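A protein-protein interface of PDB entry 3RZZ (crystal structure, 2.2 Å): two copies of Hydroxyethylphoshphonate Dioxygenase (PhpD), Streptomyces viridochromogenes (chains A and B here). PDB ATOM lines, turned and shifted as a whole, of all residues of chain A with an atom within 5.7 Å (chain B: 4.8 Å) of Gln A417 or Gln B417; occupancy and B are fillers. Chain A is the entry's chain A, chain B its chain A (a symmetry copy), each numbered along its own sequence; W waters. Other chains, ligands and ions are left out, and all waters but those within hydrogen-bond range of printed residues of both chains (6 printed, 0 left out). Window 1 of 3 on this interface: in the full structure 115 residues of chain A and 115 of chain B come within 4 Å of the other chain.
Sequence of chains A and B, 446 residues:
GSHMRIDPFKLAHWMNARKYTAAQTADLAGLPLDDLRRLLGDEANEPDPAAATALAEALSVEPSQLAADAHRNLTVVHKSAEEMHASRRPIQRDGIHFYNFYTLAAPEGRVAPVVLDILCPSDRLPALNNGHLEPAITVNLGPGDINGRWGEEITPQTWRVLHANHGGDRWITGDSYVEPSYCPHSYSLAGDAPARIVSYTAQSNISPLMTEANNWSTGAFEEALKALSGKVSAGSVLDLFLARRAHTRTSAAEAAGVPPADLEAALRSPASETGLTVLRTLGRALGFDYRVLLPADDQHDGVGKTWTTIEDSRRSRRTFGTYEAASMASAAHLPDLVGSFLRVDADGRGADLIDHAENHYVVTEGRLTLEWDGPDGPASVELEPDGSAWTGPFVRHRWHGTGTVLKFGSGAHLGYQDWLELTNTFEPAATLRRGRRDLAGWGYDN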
ATOM      1  N   ASN A 205      -7.457 -17.223   8.911  1.00  0.00           N
ATOM      2  CA  ASN A 205      -6.561 -18.076   8.145  1.00  0.00           C
ATOM      3  C   ASN A 205      -5.120 -17.982   8.623  1.00  0.00           C
ATOM      4  O   ASN A 205      -4.256 -18.735   8.175  1.00  0.00           O
ATOM      5  CB  ASN A 205      -6.661 -17.713   6.662  1.00  0.00           C
ATOM      6  CG  ASN A 205      -7.950 -18.215   6.035  1.00  0.00           C
ATOM      7  OD1 ASN A 205      -8.494 -17.600   5.120  1.00  0.00           O
ATOM      8  ND2 ASN A 205      -8.439 -19.348   6.525  1.00  0.00           N
ATOM      9  N   VAL A 292       2.399 -17.645  -5.122  1.00  0.00           N
ATOM     10  CA  VAL A 292       2.410 -16.903  -3.864  1.00  0.00           C
ATOM     11  C   VAL A 292       3.400 -15.745  -3.930  1.00  0.00           C
ATOM     12  O   VAL A 292       3.532 -14.966  -2.984  1.00  0.00           O
ATOM     13  CB  VAL A 292       2.747 -17.806  -2.632  1.00  0.00           C
ATOM     14  CG1 VAL A 292       1.688 -18.876  -2.463  1.00  0.00           C
ATOM     15  CG2 VAL A 292       4.117 -18.431  -2.783  1.00  0.00           C
ATOM     16  N   ASP A 336     -12.393 -16.072   1.860  1.00  0.00           N
ATOM     17  CA  ASP A 336     -13.297 -17.042   2.471  1.00  0.00           C
ATOM     18  C   ASP A 336     -14.486 -16.413   3.184  1.00  0.00           C
ATOM     19  O   ASP A 336     -15.373 -17.125   3.655  1.00  0.00           O
ATOM     20  CB  ASP A 336     -12.533 -17.932   3.456  1.00  0.00           C
ATOM     21  CG  ASP A 336     -11.371 -18.675   2.806  1.00  0.00           C
ATOM     22  OD1 ASP A 336     -11.519 -19.149   1.658  1.00  0.00           O
ATOM     23  OD2 ASP A 336     -10.311 -18.802   3.455  1.00  0.00           O
ATOM     24  N   GLY A 415     -11.362 -23.477   1.660  1.00  0.00           N
ATOM     25  CA  GLY A 415     -11.090 -22.072   1.429  1.00  0.00           C
ATOM     26  C   GLY A 415     -10.161 -21.873   0.249  1.00  0.00           C
ATOM     27  O   GLY A 415      -9.750 -22.839  -0.393  1.00  0.00           O
ATOM     28  N   TYR A 416      -9.830 -20.619  -0.040  1.00  0.00           N
ATOM     29  CA  TYR A 416      -8.958 -20.306  -1.165  1.00  0.00           C
ATOM     30  C   TYR A 416      -7.568 -20.903  -0.975  1.00  0.00           C
ATOM     31  O   TYR A 416      -6.818 -21.068  -1.936  1.00  0.00           O
ATOM     32  CB  TYR A 416      -8.877 -18.792  -1.386  1.00  0.00           C
ATOM     33  CG  TYR A 416      -7.885 -18.079  -0.497  1.00  0.00           C
ATOM     34  CD1 TYR A 416      -6.906 -17.258  -1.038  1.00  0.00           C
ATOM     35  CD2 TYR A 416      -7.932 -18.220   0.884  1.00  0.00           C
ATOM     36  CE1 TYR A 416      -5.998 -16.600  -0.232  1.00  0.00           C
ATOM     37  CE2 TYR A 416      -7.028 -17.566   1.698  1.00  0.00           C
ATOM     38  CZ  TYR A 416      -6.064 -16.757   1.135  1.00  0.00           C
ATOM     39  OH  TYR A 416      -5.161 -16.104   1.941  1.00  0.00           O
ATOM     40  N   GLN A 417      -7.234 -21.233   0.268  1.00  0.00           N
ATOM     41  CA  GLN A 417      -5.952 -21.857   0.576  1.00  0.00           C
ATOM     42  C   GLN A 417      -5.954 -23.317   0.139  1.00  0.00           C
ATOM     43  O   GLN A 417      -4.943 -23.835  -0.332  1.00  0.00           O
ATOM     44  CB  GLN A 417      -5.648 -21.752   2.070  1.00  0.00           C
ATOM     45  CG  GLN A 417      -4.657 -20.657   2.424  1.00  0.00           C
ATOM     46  CD  GLN A 417      -4.727 -20.259   3.883  1.00  0.00           C
ATOM     47  OE1 GLN A 417      -5.794 -20.281   4.494  1.00  0.00           O
ATOM     48  NE2 GLN A 417      -3.585 -19.892   4.451  1.00  0.00           N
ATOM     49  N   ASP A 418      -7.098 -23.973   0.295  1.00  0.00           N
ATOM     50  CA  ASP A 418      -7.252 -25.356  -0.135  1.00  0.00           C
ATOM     51  C   ASP A 418      -7.258 -25.428  -1.655  1.00  0.00           C
ATOM     52  O   ASP A 418      -6.714 -26.358  -2.248  1.00  0.00           O
ATOM     53  CB  ASP A 418      -8.550 -25.947   0.418  1.00  0.00           C
ATOM     54  CG  ASP A 418      -8.384 -26.518   1.810  1.00  0.00           C
ATOM     55  OD1 ASP A 418      -7.229 -26.710   2.242  1.00  0.00           O
ATOM     56  OD2 ASP A 418      -9.410 -26.775   2.473  1.00  0.00           O
ATOM     57  N   TRP A 419      -7.878 -24.432  -2.281  1.00  0.00           N
ATOM     58  CA  TRP A 419      -7.965 -24.372  -3.733  1.00  0.00           C
ATOM     59  C   TRP A 419      -6.587 -24.221  -4.367  1.00  0.00           C
ATOM     60  O   TRP A 419      -6.388 -24.577  -5.527  1.00  0.00           O
ATOM     61  CB  TRP A 419      -8.871 -23.219  -4.169  1.00  0.00           C
ATOM     62  CG  TRP A 419     -10.332 -23.534  -4.070  1.00  0.00           C
ATOM     63  CD1 TRP A 419     -11.254 -22.900  -3.291  1.00  0.00           C
ATOM     64  CD2 TRP A 419     -11.039 -24.559  -4.775  1.00  0.00           C
ATOM     65  NE1 TRP A 419     -12.491 -23.467  -3.467  1.00  0.00           N
ATOM     66  CE2 TRP A 419     -12.387 -24.489  -4.372  1.00  0.00           C
ATOM     67  CE3 TRP A 419     -10.663 -25.531  -5.706  1.00  0.00           C
ATOM     68  CZ2 TRP A 419     -13.360 -25.353  -4.870  1.00  0.00           C
ATOM     69  CZ3 TRP A 419     -11.631 -26.388  -6.199  1.00  0.00           C
ATOM     70  CH2 TRP A 419     -12.963 -26.293  -5.780  1.00  0.00           C
ATOM     71  N   LEU A 420      -5.638 -23.692  -3.602  1.00  0.00           N
ATOM     72  CA  LEU A 420      -4.285 -23.499  -4.109  1.00  0.00           C
ATOM     73  C   LEU A 420      -3.576 -24.854  -4.100  1.00  0.00           C
ATOM     74  O   LEU A 420      -2.846 -25.188  -5.034  1.00  0.00           O
ATOM     75  CB  LEU A 420      -3.516 -22.476  -3.255  1.00  0.00           C
ATOM     76  CG  LEU A 420      -2.136 -22.106  -3.825  1.00  0.00           C
ATOM     77  CD1 LEU A 420      -2.319 -21.527  -5.207  1.00  0.00           C
ATOM     78  CD2 LEU A 420      -1.416 -21.117  -2.938  1.00  0.00           C
ATOM     79  N   GLU A 421      -3.809 -25.639  -3.051  1.00  0.00           N
ATOM     80  CA  GLU A 421      -3.209 -26.971  -2.934  1.00  0.00           C
ATOM     81  C   GLU A 421      -3.906 -27.942  -3.891  1.00  0.00           C
ATOM     82  O   GLU A 421      -3.292 -28.867  -4.426  1.00  0.00           O
ATOM     83  CB  GLU A 421      -3.351 -27.477  -1.498  1.00  0.00           C
ATOM     84  CG  GLU A 421      -3.021 -28.947  -1.299  1.00  0.00           C
ATOM     85  CD  GLU A 421      -1.533 -29.245  -1.326  1.00  0.00           C
ATOM     86  OE1 GLU A 421      -0.713 -28.307  -1.437  1.00  0.00           O
ATOM     87  OE2 GLU A 421      -1.185 -30.435  -1.225  1.00  0.00           O
ATOM     88  N   LEU A 422      -5.198 -27.723  -4.103  1.00  0.00           N
ATOM     89  CA  LEU A 422      -5.960 -28.584  -4.985  1.00  0.00           C
ATOM     90  C   LEU A 422      -5.504 -28.439  -6.434  1.00  0.00           C
ATOM     91  O   LEU A 422      -5.408 -29.437  -7.158  1.00  0.00           O
ATOM     92  CB  LEU A 422      -7.456 -28.305  -4.824  1.00  0.00           C
ATOM     93  CG  LEU A 422      -8.003 -28.811  -3.471  1.00  0.00           C
ATOM     94  CD1 LEU A 422      -9.449 -28.417  -3.301  1.00  0.00           C
ATOM     95  CD2 LEU A 422      -7.865 -30.340  -3.393  1.00  0.00           C
ATOM     96  N   ASN B 205      -0.438 -31.348   2.664  1.00  0.00           N
ATOM     97  CA  ASN B 205      -1.171 -30.091   2.700  1.00  0.00           C
ATOM     98  C   ASN B 205      -2.645 -30.269   2.375  1.00  0.00           C
ATOM     99  O   ASN B 205      -3.436 -29.333   2.492  1.00  0.00           O
ATOM    100  CB  ASN B 205      -0.523 -29.098   1.733  1.00  0.00           C
ATOM    101  CG  ASN B 205       0.787 -28.547   2.270  1.00  0.00           C
ATOM    102  OD1 ASN B 205       1.704 -28.236   1.514  1.00  0.00           O
ATOM    103  ND2 ASN B 205       0.871 -28.414   3.589  1.00  0.00           N
ATOM    104  N   GLY B 415       4.429 -22.714   5.615  1.00  0.00           N
ATOM    105  CA  GLY B 415       4.510 -23.246   4.268  1.00  0.00           C
ATOM    106  C   GLY B 415       4.076 -22.222   3.240  1.00  0.00           C
ATOM    107  O   GLY B 415       3.730 -21.094   3.588  1.00  0.00           O
ATOM    108  N   TYR B 416       4.093 -22.614   1.971  1.00  0.00           N
ATOM    109  CA  TYR B 416       3.713 -21.708   0.893  1.00  0.00           C
ATOM    110  C   TYR B 416       2.254 -21.282   1.012  1.00  0.00           C
ATOM    111  O   TYR B 416       1.846 -20.270   0.444  1.00  0.00           O
ATOM    112  CB  TYR B 416       3.988 -22.343  -0.474  1.00  0.00           C
ATOM    113  CG  TYR B 416       2.906 -23.278  -0.961  1.00  0.00           C
ATOM    114  CD1 TYR B 416       2.327 -23.108  -2.211  1.00  0.00           C
ATOM    115  CD2 TYR B 416       2.468 -24.337  -0.176  1.00  0.00           C
ATOM    116  CE1 TYR B 416       1.341 -23.961  -2.665  1.00  0.00           C
ATOM    117  CE2 TYR B 416       1.482 -25.195  -0.621  1.00  0.00           C
ATOM    118  CZ  TYR B 416       0.922 -25.002  -1.866  1.00  0.00           C
ATOM    119  OH  TYR B 416      -0.061 -25.853  -2.315  1.00  0.00           O
ATOM    120  N   GLN B 417       1.475 -22.054   1.761  1.00  0.00           N
ATOM    121  CA  GLN B 417       0.072 -21.730   1.994  1.00  0.00           C
ATOM    122  C   GLN B 417      -0.049 -20.573   2.978  1.00  0.00           C
ATOM    123  O   GLN B 417      -0.925 -19.720   2.845  1.00  0.00           O
ATOM    124  CB  GLN B 417      -0.684 -22.951   2.517  1.00  0.00           C
ATOM    125  CG  GLN B 417      -1.518 -23.659   1.465  1.00  0.00           C
ATOM    126  CD  GLN B 417      -1.862 -25.081   1.855  1.00  0.00           C
ATOM    127  OE1 GLN B 417      -1.079 -25.763   2.515  1.00  0.00           O
ATOM    128  NE2 GLN B 417      -3.040 -25.537   1.448  1.00  0.00           N
ATOM    129  N   ASP B 418       0.839 -20.549   3.966  1.00  0.00           N
ATOM    130  CA  ASP B 418       0.872 -19.468   4.941  1.00  0.00           C
ATOM    131  C   ASP B 418       1.365 -18.189   4.280  1.00  0.00           C
ATOM    132  O   ASP B 418       0.887 -17.096   4.579  1.00  0.00           O
ATOM    133  CB  ASP B 418       1.783 -19.832   6.114  1.00  0.00           C
ATOM    134  CG  ASP B 418       1.066 -20.625   7.186  1.00  0.00           C
ATOM    135  OD1 ASP B 418      -0.181 -20.661   7.166  1.00  0.00           O
ATOM    136  OD2 ASP B 418       1.751 -21.212   8.048  1.00  0.00           O
ATOM    137  N   TRP B 419       2.327 -18.338   3.375  1.00  0.00           N
ATOM    138  CA  TRP B 419       2.898 -17.201   2.666  1.00  0.00           C
ATOM    139  C   TRP B 419       1.859 -16.515   1.787  1.00  0.00           C
ATOM    140  O   TRP B 419       1.992 -15.337   1.461  1.00  0.00           O
ATOM    141  CB  TRP B 419       4.092 -17.644   1.817  1.00  0.00           C
ATOM    142  CG  TRP B 419       5.354 -17.818   2.602  1.00  0.00           C
ATOM    143  CD1 TRP B 419       6.067 -18.970   2.759  1.00  0.00           C
ATOM    144  CD2 TRP B 419       6.054 -16.810   3.338  1.00  0.00           C
ATOM    145  NE1 TRP B 419       7.168 -18.741   3.546  1.00  0.00           N
ATOM    146  CE2 TRP B 419       7.183 -17.423   3.916  1.00  0.00           C
ATOM    147  CE3 TRP B 419       5.836 -15.448   3.565  1.00  0.00           C
ATOM    148  CZ2 TRP B 419       8.091 -16.720   4.706  1.00  0.00           C
ATOM    149  CZ3 TRP B 419       6.739 -14.753   4.350  1.00  0.00           C
ATOM    150  CH2 TRP B 419       7.852 -15.390   4.910  1.00  0.00           C
ATOM    151  N   LEU B 420       0.824 -17.256   1.405  1.00  0.00           N
ATOM    152  CA  LEU B 420      -0.227 -16.702   0.561  1.00  0.00           C
ATOM    153  C   LEU B 420      -1.134 -15.836   1.437  1.00  0.00           C
ATOM    154  O   LEU B 420      -1.564 -14.758   1.026  1.00  0.00           O
ATOM    155  CB  LEU B 420      -1.034 -17.819  -0.122  1.00  0.00           C
ATOM    156  CG  LEU B 420      -2.057 -17.305  -1.149  1.00  0.00           C
ATOM    157  CD1 LEU B 420      -1.325 -16.528  -2.218  1.00  0.00           C
ATOM    158  CD2 LEU B 420      -2.836 -18.439  -1.773  1.00  0.00           C
ATOM    159  N   GLU B 421      -1.408 -16.305   2.653  1.00  0.00           N
ATOM    160  CA  GLU B 421      -2.245 -15.561   3.597  1.00  0.00           C
ATOM    161  C   GLU B 421      -1.461 -14.374   4.165  1.00  0.00           C
ATOM    162  O   GLU B 421      -2.022 -13.318   4.465  1.00  0.00           O
ATOM    163  CB  GLU B 421      -2.680 -16.481   4.739  1.00  0.00           C
ATOM    164  CG  GLU B 421      -3.319 -15.777   5.924  1.00  0.00           C
ATOM    165  CD  GLU B 421      -4.743 -15.320   5.663  1.00  0.00           C
ATOM    166  OE1 GLU B 421      -5.294 -15.594   4.575  1.00  0.00           O
ATOM    167  OE2 GLU B 421      -5.316 -14.686   6.568  1.00  0.00           O
HETATM  168  O   HOH W   1       1.696 -29.438  -1.362  1.00  0.00           O
HETATM  169  O   HOH W   2      -8.161 -14.797   7.711  1.00  0.00           O
HETATM  170  O   HOH W   3      -6.286 -29.154   3.700  1.00  0.00           O
HETATM  171  O   HOH W   4      -7.757 -14.595   4.739  1.00  0.00           O
HETATM  172  O   HOH W   5      -1.982 -20.340   9.542  1.00  0.00           O
HETATM  173  O   HOH W   6       1.054 -31.827   0.346  1.00  0.00           O
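Hydrophobic or aromatic side chains of chain B that line the printed part of chain A: Tyr B416 and Leu B420. Of the 11 printed residues of chain A, 6 touch a printed residue of chain B. Hydrophobic or aromatic side chains of chain A within 4 Å of the printed part of chain B: Val A292, Tyr A416 and Leu A420. Among the printed residues, 12 pairs touch across the chains.
Water W4 bridges the side-chain carboxylate (OE1) of Glu B421 (2.7 Å) and the side-chain amide oxygen (OD1) of Asn A205 (3.1 Å). Water W1 lies within hydrogen-bond range of the side-chain carboxylate (OE1) of Glu A421 (2.7 Å) and the side-chain amide oxygen (OD1) of Asn B205 (3.1 Å). Water W2 bridges N of Asn A205 (2.8 Å) and OE2 of Glu B421 (3.1 Å). Water W6 lies within hydrogen-bond range of N of Asn B205 (2.8 Å) and OE2 of Glu A421 (3.1 Å). Water W3 lies within hydrogen-bond range of OD1 of Asp A418 and O of Asn B205. Water W5 bridges OD1 of Asp B418 (3.0 Å) and O of Asn A205 (3.1 Å).
Among the printed residues, merely in contact across the chains: Glu A421 with Asn B205 (3.2 Å), Asn A205 with Glu B421 (3.2 Å), Val A292 with Tyr B416 (3.2 Å), Leu A420 with Leu B420 (3.2 Å), Gln A417 with Glu B421 (3.5 Å), Glu A421 with Gln B417 (3.5 Å), Val A292 with Leu B420 (3.7 Å), Tyr A416 with Leu B420 (3.9 Å) and Leu A420 with Tyr B416 (3.9 Å).
Asn A205 touches Glu B421, and with the chains exchanged Glu A421 touches Asn B205. Tyr A416 touches Glu B421, and with the chains exchanged Glu A421 touches Tyr B416. Gln A417 touches its own counterpart, Gln B417. Gln A417 touches Glu B421, and with the chains exchanged Glu A421 touches Gln B417.
Gln A417 touches just these residues of chain B: Gln B417 (3.1 Å) and Glu B421 (3.5 Å). Gln B417 touches just these residues of chain A: Gln A417 (3.1 Å) and Glu A421 (3.5 Å). Of the printed residues of chain B, Asn A205 touches Glu B421 (3.2 Å). Printed residues of chain B within 4 Å of Glu A421: Asn B205, Tyr B416 and Gln B417. Leu A422 touches none of the printed residues of chain B. Trp A419 touches none of the printed residues of chain B. The nearest residue of chain A that does not touch Gln B417 is Asp A418 (4.4 Å).
The side-chain carboxylate of Glu B421 lies within hydrogen-bond range of the side-chain hydroxyl of Tyr A416, at 2.7 Å. O of Gln A417 lies within hydrogen-bond range of NE2 of Gln B417 (3.1 Å). The side-chain carboxylate (OE1) of Glu A421 lies within hydrogen-bond range of the side-chain hydroxyl (OH) of Tyr B416 (2.7 Å).
OD1 of Asn A205 lies close to OD2 of Asp A336, at 2.7 Å. The side-chain amide nitrogen (ND2) of Asn A205 sits close to the side-chain amide oxygen (OE1) of Gln A417, at 3.5 Å. N of Tyr A416 sits at hydrogen-bond distance from OD1 of Asp A336, 2.8 Å away. The side-chain amide nitrogen (ND2) of Asn B205 lies close to the side-chain amide oxygen (OE1) of Gln B417, at 3.5 Å.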
